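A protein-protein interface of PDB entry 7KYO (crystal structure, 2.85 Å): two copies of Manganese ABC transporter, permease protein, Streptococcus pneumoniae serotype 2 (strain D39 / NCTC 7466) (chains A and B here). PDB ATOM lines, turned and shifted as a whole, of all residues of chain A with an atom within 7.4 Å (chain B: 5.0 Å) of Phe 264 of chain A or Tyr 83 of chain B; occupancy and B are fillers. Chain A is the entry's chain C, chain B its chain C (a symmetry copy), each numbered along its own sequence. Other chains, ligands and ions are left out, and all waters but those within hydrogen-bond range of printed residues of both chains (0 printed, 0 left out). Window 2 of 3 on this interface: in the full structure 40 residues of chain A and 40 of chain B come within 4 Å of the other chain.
O of Phe 264 of chain A sits close to OE1 of Gln 270 of chain A (3.0 Å).
O of Tyr 83 of chain B sits close to OD1 of Asn 87 of chain B (3.4 Å).
The backbone carbonyl oxygen (O) of Ile 84 of chain B is in hydrogen-bond range of the side-chain hydroxyl (OG) of Ser 88 of chain B (2.6 Å).
No position is printed for both chains.
Of the 6 pairs that touch across the chains among the printed residues, none has its exchanged pair printed and touching as well.
CE2 of Tyr 83 of chain B touches CE2 of Phe 264 of chain A (3.9 Å).
Ile 84 of chain B touches Phe 264 of chain A (CA to CZ, 3.8 Å).
Asn 87 of chain B touches Phe 264 of chain A.
Phe 264 of chain A touches Ser 88 of chain B.
NE2 of Gln 270 of chain A touches CB of Ser 88 of chain B (3.7 Å).
Of the 10 printed residues of chain B, 4 touch a printed residue of chain A.
Hydrophobic or aromatic side chains of chain B within 4 Å of the printed part of chain A: Tyr 83.
Of the 16 printed residues of chain A, 2 touch a printed residue of chain B.
Printed residues of chain A that touch a printed residue of chain B: Phe 264 and Gln 270.
Among the printed residues, 6 pairs touch across the chains.
Among the printed residues, no Asp or Glu carboxylate lies within 4 Å of a Lys or Arg side-chain nitrogen of the other chain.
Tyr 215 of chain A touches none of the printed residues of chain B.
Phe 264 of chain A touches just these residues of chain B: Tyr 83 (3.9 Å), Ile 84 (3.8 Å), Asn 87 (3.8 Å) and Ser 88 (3.4 Å).
Lys 269 of chain A touches none of the printed residues of chain B.
Printed residues of chain B within 4 Å of Gln 270 of chain A: Asn 87 and Ser 88.
Tyr 83 of chain B touches one residue of chain A.
Of the printed residues of chain A, Ile 84 of chain B touches Phe 264 (3.8 Å).
Of the printed residues of chain A, Asn 87 of chain B touches Phe 264 and Gln 270.
Of the printed residues of chain A, Ser 88 of chain B touches Phe 264 and Gln 270.
The nearest residue of chain A that does not touch Tyr 83 of chain B is Phe 265 of chain A (4.2 Å).
The nearest printed residue of chain B that does not touch Gln 270 of chain A is Ile 84 of chain B (6.6 Å).
OE1 of Gln 270 of chain A lies close to O of Asn 87 of chain B (2.9 Å).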
ATOM      1  N   ALA A 210     -18.172  -4.864  -3.021  1.00  0.00           N
ATOM      2  CA  ALA A 210     -18.183  -3.825  -1.983  1.00  0.00           C
ATOM      3  C   ALA A 210     -18.798  -2.517  -2.481  1.00  0.00           C
ATOM      4  O   ALA A 210     -19.491  -1.838  -1.724  1.00  0.00           O
ATOM      5  CB  ALA A 210     -16.775  -3.575  -1.464  1.00  0.00           C
ATOM      6  N   THR A 211     -18.533  -2.172  -3.743  1.00  0.00           N
ATOM      7  CA  THR A 211     -19.148  -1.003  -4.384  1.00  0.00           C
ATOM      8  C   THR A 211     -20.663  -1.176  -4.494  1.00  0.00           C
ATOM      9  O   THR A 211     -21.422  -0.286  -4.113  1.00  0.00           O
ATOM     10  CB  THR A 211     -18.581  -0.760  -5.801  1.00  0.00           C
ATOM     11  OG1 THR A 211     -17.150  -0.786  -5.766  1.00  0.00           O
ATOM     12  CG2 THR A 211     -19.049   0.588  -6.358  1.00  0.00           C
ATOM     13  N   LEU A 214     -22.806  -0.829  -1.255  1.00  0.00           N
ATOM     14  CA  LEU A 214     -23.167   0.527  -0.832  1.00  0.00           C
ATOM     15  C   LEU A 214     -24.520   0.982  -1.392  1.00  0.00           C
ATOM     16  O   LEU A 214     -25.226   1.744  -0.731  1.00  0.00           O
ATOM     17  CB  LEU A 214     -22.083   1.533  -1.235  1.00  0.00           C
ATOM     18  CG  LEU A 214     -20.671   1.307  -0.675  1.00  0.00           C
ATOM     19  CD1 LEU A 214     -19.707   2.298  -1.308  1.00  0.00           C
ATOM     20  CD2 LEU A 214     -20.631   1.388   0.849  1.00  0.00           C
ATOM     21  N   TYR A 215     -24.865   0.523  -2.600  1.00  0.00           N
ATOM     22  CA  TYR A 215     -26.145   0.865  -3.249  1.00  0.00           C
ATOM     23  C   TYR A 215     -27.268  -0.141  -2.999  1.00  0.00           C
ATOM     24  O   TYR A 215     -28.430   0.248  -2.899  1.00  0.00           O
ATOM     25  CB  TYR A 215     -25.964   0.985  -4.766  1.00  0.00           C
ATOM     26  CG  TYR A 215     -25.011   2.067  -5.205  1.00  0.00           C
ATOM     27  CD1 TYR A 215     -25.435   3.390  -5.332  1.00  0.00           C
ATOM     28  CD2 TYR A 215     -23.687   1.767  -5.512  1.00  0.00           C
ATOM     29  CE1 TYR A 215     -24.560   4.386  -5.744  1.00  0.00           C
ATOM     30  CE2 TYR A 215     -22.804   2.752  -5.925  1.00  0.00           C
ATOM     31  CZ  TYR A 215     -23.242   4.059  -6.037  1.00  0.00           C
ATOM     32  OH  TYR A 215     -22.367   5.037  -6.443  1.00  0.00           O
ATOM     33  N   SER A 258     -11.323   3.253  -7.694  1.00  0.00           N
ATOM     34  CA  SER A 258     -11.864   4.604  -7.878  1.00  0.00           C
ATOM     35  C   SER A 258     -13.390   4.595  -8.019  1.00  0.00           C
ATOM     36  O   SER A 258     -14.051   5.547  -7.600  1.00  0.00           O
ATOM     37  CB  SER A 258     -11.224   5.287  -9.089  1.00  0.00           C
ATOM     38  OG  SER A 258     -11.579   4.634 -10.293  1.00  0.00           O
ATOM     39  N   PHE A 259     -13.939   3.536  -8.621  1.00  0.00           N
ATOM     40  CA  PHE A 259     -15.397   3.305  -8.654  1.00  0.00           C
ATOM     41  C   PHE A 259     -15.970   3.189  -7.237  1.00  0.00           C
ATOM     42  O   PHE A 259     -17.004   3.784  -6.932  1.00  0.00           O
ATOM     43  CB  PHE A 259     -15.743   2.038  -9.463  1.00  0.00           C
ATOM     44  CG  PHE A 259     -15.889   2.258 -10.951  1.00  0.00           C
ATOM     45  CD1 PHE A 259     -15.214   3.284 -11.620  1.00  0.00           C
ATOM     46  CD2 PHE A 259     -16.691   1.400 -11.696  1.00  0.00           C
ATOM     47  CE1 PHE A 259     -15.364   3.455 -12.990  1.00  0.00           C
ATOM     48  CE2 PHE A 259     -16.840   1.565 -13.064  1.00  0.00           C
ATOM     49  CZ  PHE A 259     -16.176   2.593 -13.712  1.00  0.00           C
ATOM     50  N   PHE A 260     -15.287   2.422  -6.387  1.00  0.00           N
ATOM     51  CA  PHE A 260     -15.632   2.310  -4.966  1.00  0.00           C
ATOM     52  C   PHE A 260     -15.479   3.652  -4.242  1.00  0.00           C
ATOM     53  O   PHE A 260     -16.361   4.046  -3.481  1.00  0.00           O
ATOM     54  CB  PHE A 260     -14.759   1.235  -4.297  1.00  0.00           C
ATOM     55  CG  PHE A 260     -15.029   1.045  -2.827  1.00  0.00           C
ATOM     56  CD1 PHE A 260     -16.134   0.319  -2.397  1.00  0.00           C
ATOM     57  CD2 PHE A 260     -14.165   1.577  -1.870  1.00  0.00           C
ATOM     58  CE1 PHE A 260     -16.381   0.138  -1.042  1.00  0.00           C
ATOM     59  CE2 PHE A 260     -14.406   1.399  -0.516  1.00  0.00           C
ATOM     60  CZ  PHE A 260     -15.516   0.679  -0.100  1.00  0.00           C
ATOM     61  N   LEU A 261     -14.366   4.343  -4.497  1.00  0.00           N
ATOM     62  CA  LEU A 261     -14.062   5.636  -3.864  1.00  0.00           C
ATOM     63  C   LEU A 261     -15.061   6.738  -4.231  1.00  0.00           C
ATOM     64  O   LEU A 261     -15.449   7.532  -3.372  1.00  0.00           O
ATOM     65  CB  LEU A 261     -12.638   6.085  -4.233  1.00  0.00           C
ATOM     66  CG  LEU A 261     -12.087   7.373  -3.605  1.00  0.00           C
ATOM     67  CD1 LEU A 261     -12.152   7.323  -2.083  1.00  0.00           C
ATOM     68  CD2 LEU A 261     -10.659   7.612  -4.074  1.00  0.00           C
ATOM     69  N   ILE A 262     -15.456   6.787  -5.504  1.00  0.00           N
ATOM     70  CA  ILE A 262     -16.501   7.707  -5.970  1.00  0.00           C
ATOM     71  C   ILE A 262     -17.848   7.326  -5.348  1.00  0.00           C
ATOM     72  O   ILE A 262     -18.559   8.187  -4.825  1.00  0.00           O
ATOM     73  CB  ILE A 262     -16.595   7.731  -7.521  1.00  0.00           C
ATOM     74  CG1 ILE A 262     -15.348   8.395  -8.121  1.00  0.00           C
ATOM     75  CG2 ILE A 262     -17.837   8.478  -7.997  1.00  0.00           C
ATOM     76  CD1 ILE A 262     -15.093   8.042  -9.573  1.00  0.00           C
ATOM     77  N   SER A 263     -18.182   6.036  -5.401  1.00  0.00           N
ATOM     78  CA  SER A 263     -19.430   5.513  -4.823  1.00  0.00           C
ATOM     79  C   SER A 263     -19.545   5.693  -3.304  1.00  0.00           C
ATOM     80  O   SER A 263     -20.654   5.800  -2.783  1.00  0.00           O
ATOM     81  CB  SER A 263     -19.596   4.029  -5.164  1.00  0.00           C
ATOM     82  OG  SER A 263     -19.695   3.833  -6.563  1.00  0.00           O
ATOM     83  N   PHE A 264     -18.408   5.721  -2.605  1.00  0.00           N
ATOM     84  CA  PHE A 264     -18.382   5.920  -1.151  1.00  0.00           C
ATOM     85  C   PHE A 264     -19.001   7.252  -0.709  1.00  0.00           C
ATOM     86  O   PHE A 264     -19.545   7.343   0.391  1.00  0.00           O
ATOM     87  CB  PHE A 264     -16.950   5.811  -0.614  1.00  0.00           C
ATOM     88  CG  PHE A 264     -16.875   5.542   0.861  1.00  0.00           C
ATOM     89  CD1 PHE A 264     -16.889   4.237   1.340  1.00  0.00           C
ATOM     90  CD2 PHE A 264     -16.791   6.590   1.774  1.00  0.00           C
ATOM     91  CE1 PHE A 264     -16.823   3.982   2.702  1.00  0.00           C
ATOM     92  CE2 PHE A 264     -16.725   6.340   3.137  1.00  0.00           C
ATOM     93  CZ  PHE A 264     -16.740   5.035   3.601  1.00  0.00           C
ATOM     94  N   PHE A 265     -18.906   8.273  -1.562  1.00  0.00           N
ATOM     95  CA  PHE A 265     -19.522   9.581  -1.313  1.00  0.00           C
ATOM     96  C   PHE A 265     -20.880   9.742  -2.005  1.00  0.00           C
ATOM     97  O   PHE A 265     -21.817  10.270  -1.405  1.00  0.00           O
ATOM     98  CB  PHE A 265     -18.574  10.699  -1.750  1.00  0.00           C
ATOM     99  CG  PHE A 265     -17.212  10.614  -1.117  1.00  0.00           C
ATOM    100  CD1 PHE A 265     -17.050  10.851   0.246  1.00  0.00           C
ATOM    101  CD2 PHE A 265     -16.089  10.283  -1.875  1.00  0.00           C
ATOM    102  CE1 PHE A 265     -15.798  10.765   0.840  1.00  0.00           C
ATOM    103  CE2 PHE A 265     -14.834  10.197  -1.287  1.00  0.00           C
ATOM    104  CZ  PHE A 265     -14.687  10.439   0.072  1.00  0.00           C
ATOM    105  N   ILE A 266     -20.983   9.284  -3.255  1.00  0.00           N
ATOM    106  CA  ILE A 266     -22.198   9.469  -4.072  1.00  0.00           C
ATOM    107  C   ILE A 266     -23.392   8.598  -3.631  1.00  0.00           C
ATOM    108  O   ILE A 266     -24.541   9.026  -3.779  1.00  0.00           O
ATOM    109  CB  ILE A 266     -21.898   9.281  -5.587  1.00  0.00           C
ATOM    110  CG1 ILE A 266     -20.940  10.387  -6.052  1.00  0.00           C
ATOM    111  CG2 ILE A 266     -23.181   9.292  -6.427  1.00  0.00           C
ATOM    112  CD1 ILE A 266     -20.582  10.356  -7.522  1.00  0.00           C
ATOM    113  N   ALA A 267     -23.129   7.400  -3.100  1.00  0.00           N
ATOM    114  CA  ALA A 267     -24.197   6.473  -2.675  1.00  0.00           C
ATOM    115  C   ALA A 267     -25.237   7.166  -1.778  1.00  0.00           C
ATOM    116  O   ALA A 267     -24.870   7.688  -0.722  1.00  0.00           O
ATOM    117  CB  ALA A 267     -23.610   5.271  -1.950  1.00  0.00           C
ATOM    118  N   LYS A 269     -27.401   6.051   0.278  1.00  0.00           N
ATOM    119  CA  LYS A 269     -27.433   5.468   1.628  1.00  0.00           C
ATOM    120  C   LYS A 269     -26.356   6.004   2.601  1.00  0.00           C
ATOM    121  O   LYS A 269     -26.381   5.659   3.784  1.00  0.00           O
ATOM    122  CB  LYS A 269     -27.386   3.932   1.550  1.00  0.00           C
ATOM    123  CG  LYS A 269     -28.642   3.326   0.932  1.00  0.00           C
ATOM    124  CD  LYS A 269     -28.538   1.825   0.678  1.00  0.00           C
ATOM    125  CE  LYS A 269     -28.452   0.998   1.956  1.00  0.00           C
ATOM    126  NZ  LYS A 269     -27.057   0.585   2.288  1.00  0.00           N
ATOM    127  N   GLN A 270     -25.420   6.823   2.113  1.00  0.00           N
ATOM    128  CA  GLN A 270     -24.524   7.605   2.977  1.00  0.00           C
ATOM    129  C   GLN A 270     -24.196   8.966   2.364  1.00  0.00           C
ATOM    130  O   GLN A 270     -24.874   9.958   2.636  1.00  0.00           O
ATOM    131  CB  GLN A 270     -23.235   6.830   3.261  1.00  0.00           C
ATOM    132  CG  GLN A 270     -22.513   6.308   2.028  1.00  0.00           C
ATOM    133  CD  GLN A 270     -21.299   5.479   2.392  1.00  0.00           C
ATOM    134  OE1 GLN A 270     -20.361   6.032   3.003  1.00  0.00           O
ATOM    135  NE2 GLN A 270     -21.279   4.275   2.068  1.00  0.00           N
ATOM    136  N   ILE B  79      -5.324   4.880   7.640  1.00  0.00           N
ATOM    137  CA  ILE B  79      -6.302   5.978   7.693  1.00  0.00           C
ATOM    138  C   ILE B  79      -7.505   5.694   6.782  1.00  0.00           C
ATOM    139  O   ILE B  79      -8.643   5.977   7.160  1.00  0.00           O
ATOM    140  CB  ILE B  79      -5.649   7.344   7.339  1.00  0.00           C
ATOM    141  CG1 ILE B  79      -4.640   7.747   8.429  1.00  0.00           C
ATOM    142  CG2 ILE B  79      -6.694   8.452   7.185  1.00  0.00           C
ATOM    143  CD1 ILE B  79      -3.587   8.733   7.969  1.00  0.00           C
ATOM    144  N   ILE B  80      -7.250   5.133   5.599  1.00  0.00           N
ATOM    145  CA  ILE B  80      -8.317   4.809   4.643  1.00  0.00           C
ATOM    146  C   ILE B  80      -9.160   3.618   5.121  1.00  0.00           C
ATOM    147  O   ILE B  80     -10.374   3.609   4.916  1.00  0.00           O
ATOM    148  CB  ILE B  80      -7.758   4.543   3.224  1.00  0.00           C
ATOM    149  CG1 ILE B  80      -7.062   5.798   2.679  1.00  0.00           C
ATOM    150  CG2 ILE B  80      -8.874   4.152   2.258  1.00  0.00           C
ATOM    151  CD1 ILE B  80      -6.062   5.515   1.579  1.00  0.00           C
ATOM    152  N   ILE B  81      -8.522   2.628   5.749  1.00  0.00           N
ATOM    153  CA  ILE B  81      -9.233   1.479   6.337  1.00  0.00           C
ATOM    154  C   ILE B  81     -10.168   1.939   7.461  1.00  0.00           C
ATOM    155  O   ILE B  81     -11.353   1.600   7.464  1.00  0.00           O
ATOM    156  CB  ILE B  81      -8.254   0.398   6.865  1.00  0.00           C
ATOM    157  CG1 ILE B  81      -7.526  -0.278   5.697  1.00  0.00           C
ATOM    158  CG2 ILE B  81      -8.983  -0.671   7.680  1.00  0.00           C
ATOM    159  CD1 ILE B  81      -6.207  -0.920   6.077  1.00  0.00           C
ATOM    160  N   THR B  82      -9.627   2.715   8.400  1.00  0.00           N
ATOM    161  CA  THR B  82     -10.399   3.245   9.534  1.00  0.00           C
ATOM    162  C   THR B  82     -11.570   4.133   9.090  1.00  0.00           C
ATOM    163  O   THR B  82     -12.623   4.127   9.726  1.00  0.00           O
ATOM    164  CB  THR B  82      -9.489   4.031  10.508  1.00  0.00           C
ATOM    165  OG1 THR B  82      -8.394   3.198  10.914  1.00  0.00           O
ATOM    166  CG2 THR B  82     -10.256   4.485  11.749  1.00  0.00           C
ATOM    167  N   TYR B  83     -11.383   4.883   8.003  1.00  0.00           N
ATOM    168  CA  TYR B  83     -12.436   5.732   7.438  1.00  0.00           C
ATOM    169  C   TYR B  83     -13.552   4.918   6.774  1.00  0.00           C
ATOM    170  O   TYR B  83     -14.727   5.264   6.912  1.00  0.00           O
ATOM    171  CB  TYR B  83     -11.842   6.728   6.435  1.00  0.00           C
ATOM    172  CG  TYR B  83     -12.787   7.845   6.046  1.00  0.00           C
ATOM    173  CD1 TYR B  83     -13.162   8.822   6.972  1.00  0.00           C
ATOM    174  CD2 TYR B  83     -13.306   7.934   4.749  1.00  0.00           C
ATOM    175  CE1 TYR B  83     -14.029   9.850   6.623  1.00  0.00           C
ATOM    176  CE2 TYR B  83     -14.173   8.961   4.389  1.00  0.00           C
ATOM    177  CZ  TYR B  83     -14.533   9.917   5.328  1.00  0.00           C
ATOM    178  OH  TYR B  83     -15.392  10.935   4.981  1.00  0.00           O
ATOM    179  N   ILE B  84     -13.188   3.850   6.060  1.00  0.00           N
ATOM    180  CA  ILE B  84     -14.171   2.956   5.420  1.00  0.00           C
ATOM    181  C   ILE B  84     -14.995   2.199   6.466  1.00  0.00           C
ATOM    182  O   ILE B  84     -16.218   2.128   6.350  1.00  0.00           O
ATOM    183  CB  ILE B  84     -13.500   1.955   4.439  1.00  0.00           C
ATOM    184  CG1 ILE B  84     -12.905   2.700   3.235  1.00  0.00           C
ATOM    185  CG2 ILE B  84     -14.497   0.910   3.934  1.00  0.00           C
ATOM    186  CD1 ILE B  84     -11.788   1.951   2.536  1.00  0.00           C
ATOM    187  N   LYS B  85     -14.323   1.634   7.470  1.00  0.00           N
ATOM    188  CA  LYS B  85     -14.999   0.936   8.577  1.00  0.00           C
ATOM    189  C   LYS B  85     -15.960   1.844   9.350  1.00  0.00           C
ATOM    190  O   LYS B  85     -17.058   1.420   9.719  1.00  0.00           O
ATOM    191  CB  LYS B  85     -13.981   0.346   9.562  1.00  0.00           C
ATOM    192  CG  LYS B  85     -13.190  -0.838   9.027  1.00  0.00           C
ATOM    193  CD  LYS B  85     -12.501  -1.617  10.143  1.00  0.00           C
ATOM    194  CE  LYS B  85     -11.460  -0.791  10.886  1.00  0.00           C
ATOM    195  NZ  LYS B  85     -10.668  -1.632  11.828  1.00  0.00           N
ATOM    196  N   GLY B  86     -15.534   3.083   9.589  1.00  0.00           N
ATOM    197  CA  GLY B  86     -16.306   4.042  10.369  1.00  0.00           C
ATOM    198  C   GLY B  86     -17.537   4.585   9.670  1.00  0.00           C
ATOM    199  O   GLY B  86     -18.613   4.634  10.268  1.00  0.00           O
ATOM    200  N   ASN B  87     -17.385   4.984   8.407  1.00  0.00           N
ATOM    201  CA  ASN B  87     -18.443   5.696   7.672  1.00  0.00           C
ATOM    202  C   ASN B  87     -19.237   4.833   6.674  1.00  0.00           C
ATOM    203  O   ASN B  87     -19.876   5.372   5.765  1.00  0.00           O
ATOM    204  CB  ASN B  87     -17.841   6.912   6.953  1.00  0.00           C
ATOM    205  CG  ASN B  87     -17.199   7.900   7.911  1.00  0.00           C
ATOM    206  OD1 ASN B  87     -16.459   7.515   8.817  1.00  0.00           O
ATOM    207  ND2 ASN B  87     -17.476   9.184   7.711  1.00  0.00           N
ATOM    208  N   SER B  88     -19.219   3.508   6.843  1.00  0.00           N
ATOM    209  CA  SER B  88     -20.029   2.609   6.009  1.00  0.00           C
ATOM    210  C   SER B  88     -20.273   1.259   6.681  1.00  0.00           C
ATOM    211  O   SER B  88     -19.703   0.966   7.735  1.00  0.00           O
ATOM    212  CB  SER B  88     -19.370   2.399   4.638  1.00  0.00           C
ATOM    213  OG  SER B  88     -18.208   1.596   4.737  1.00  0.00           O
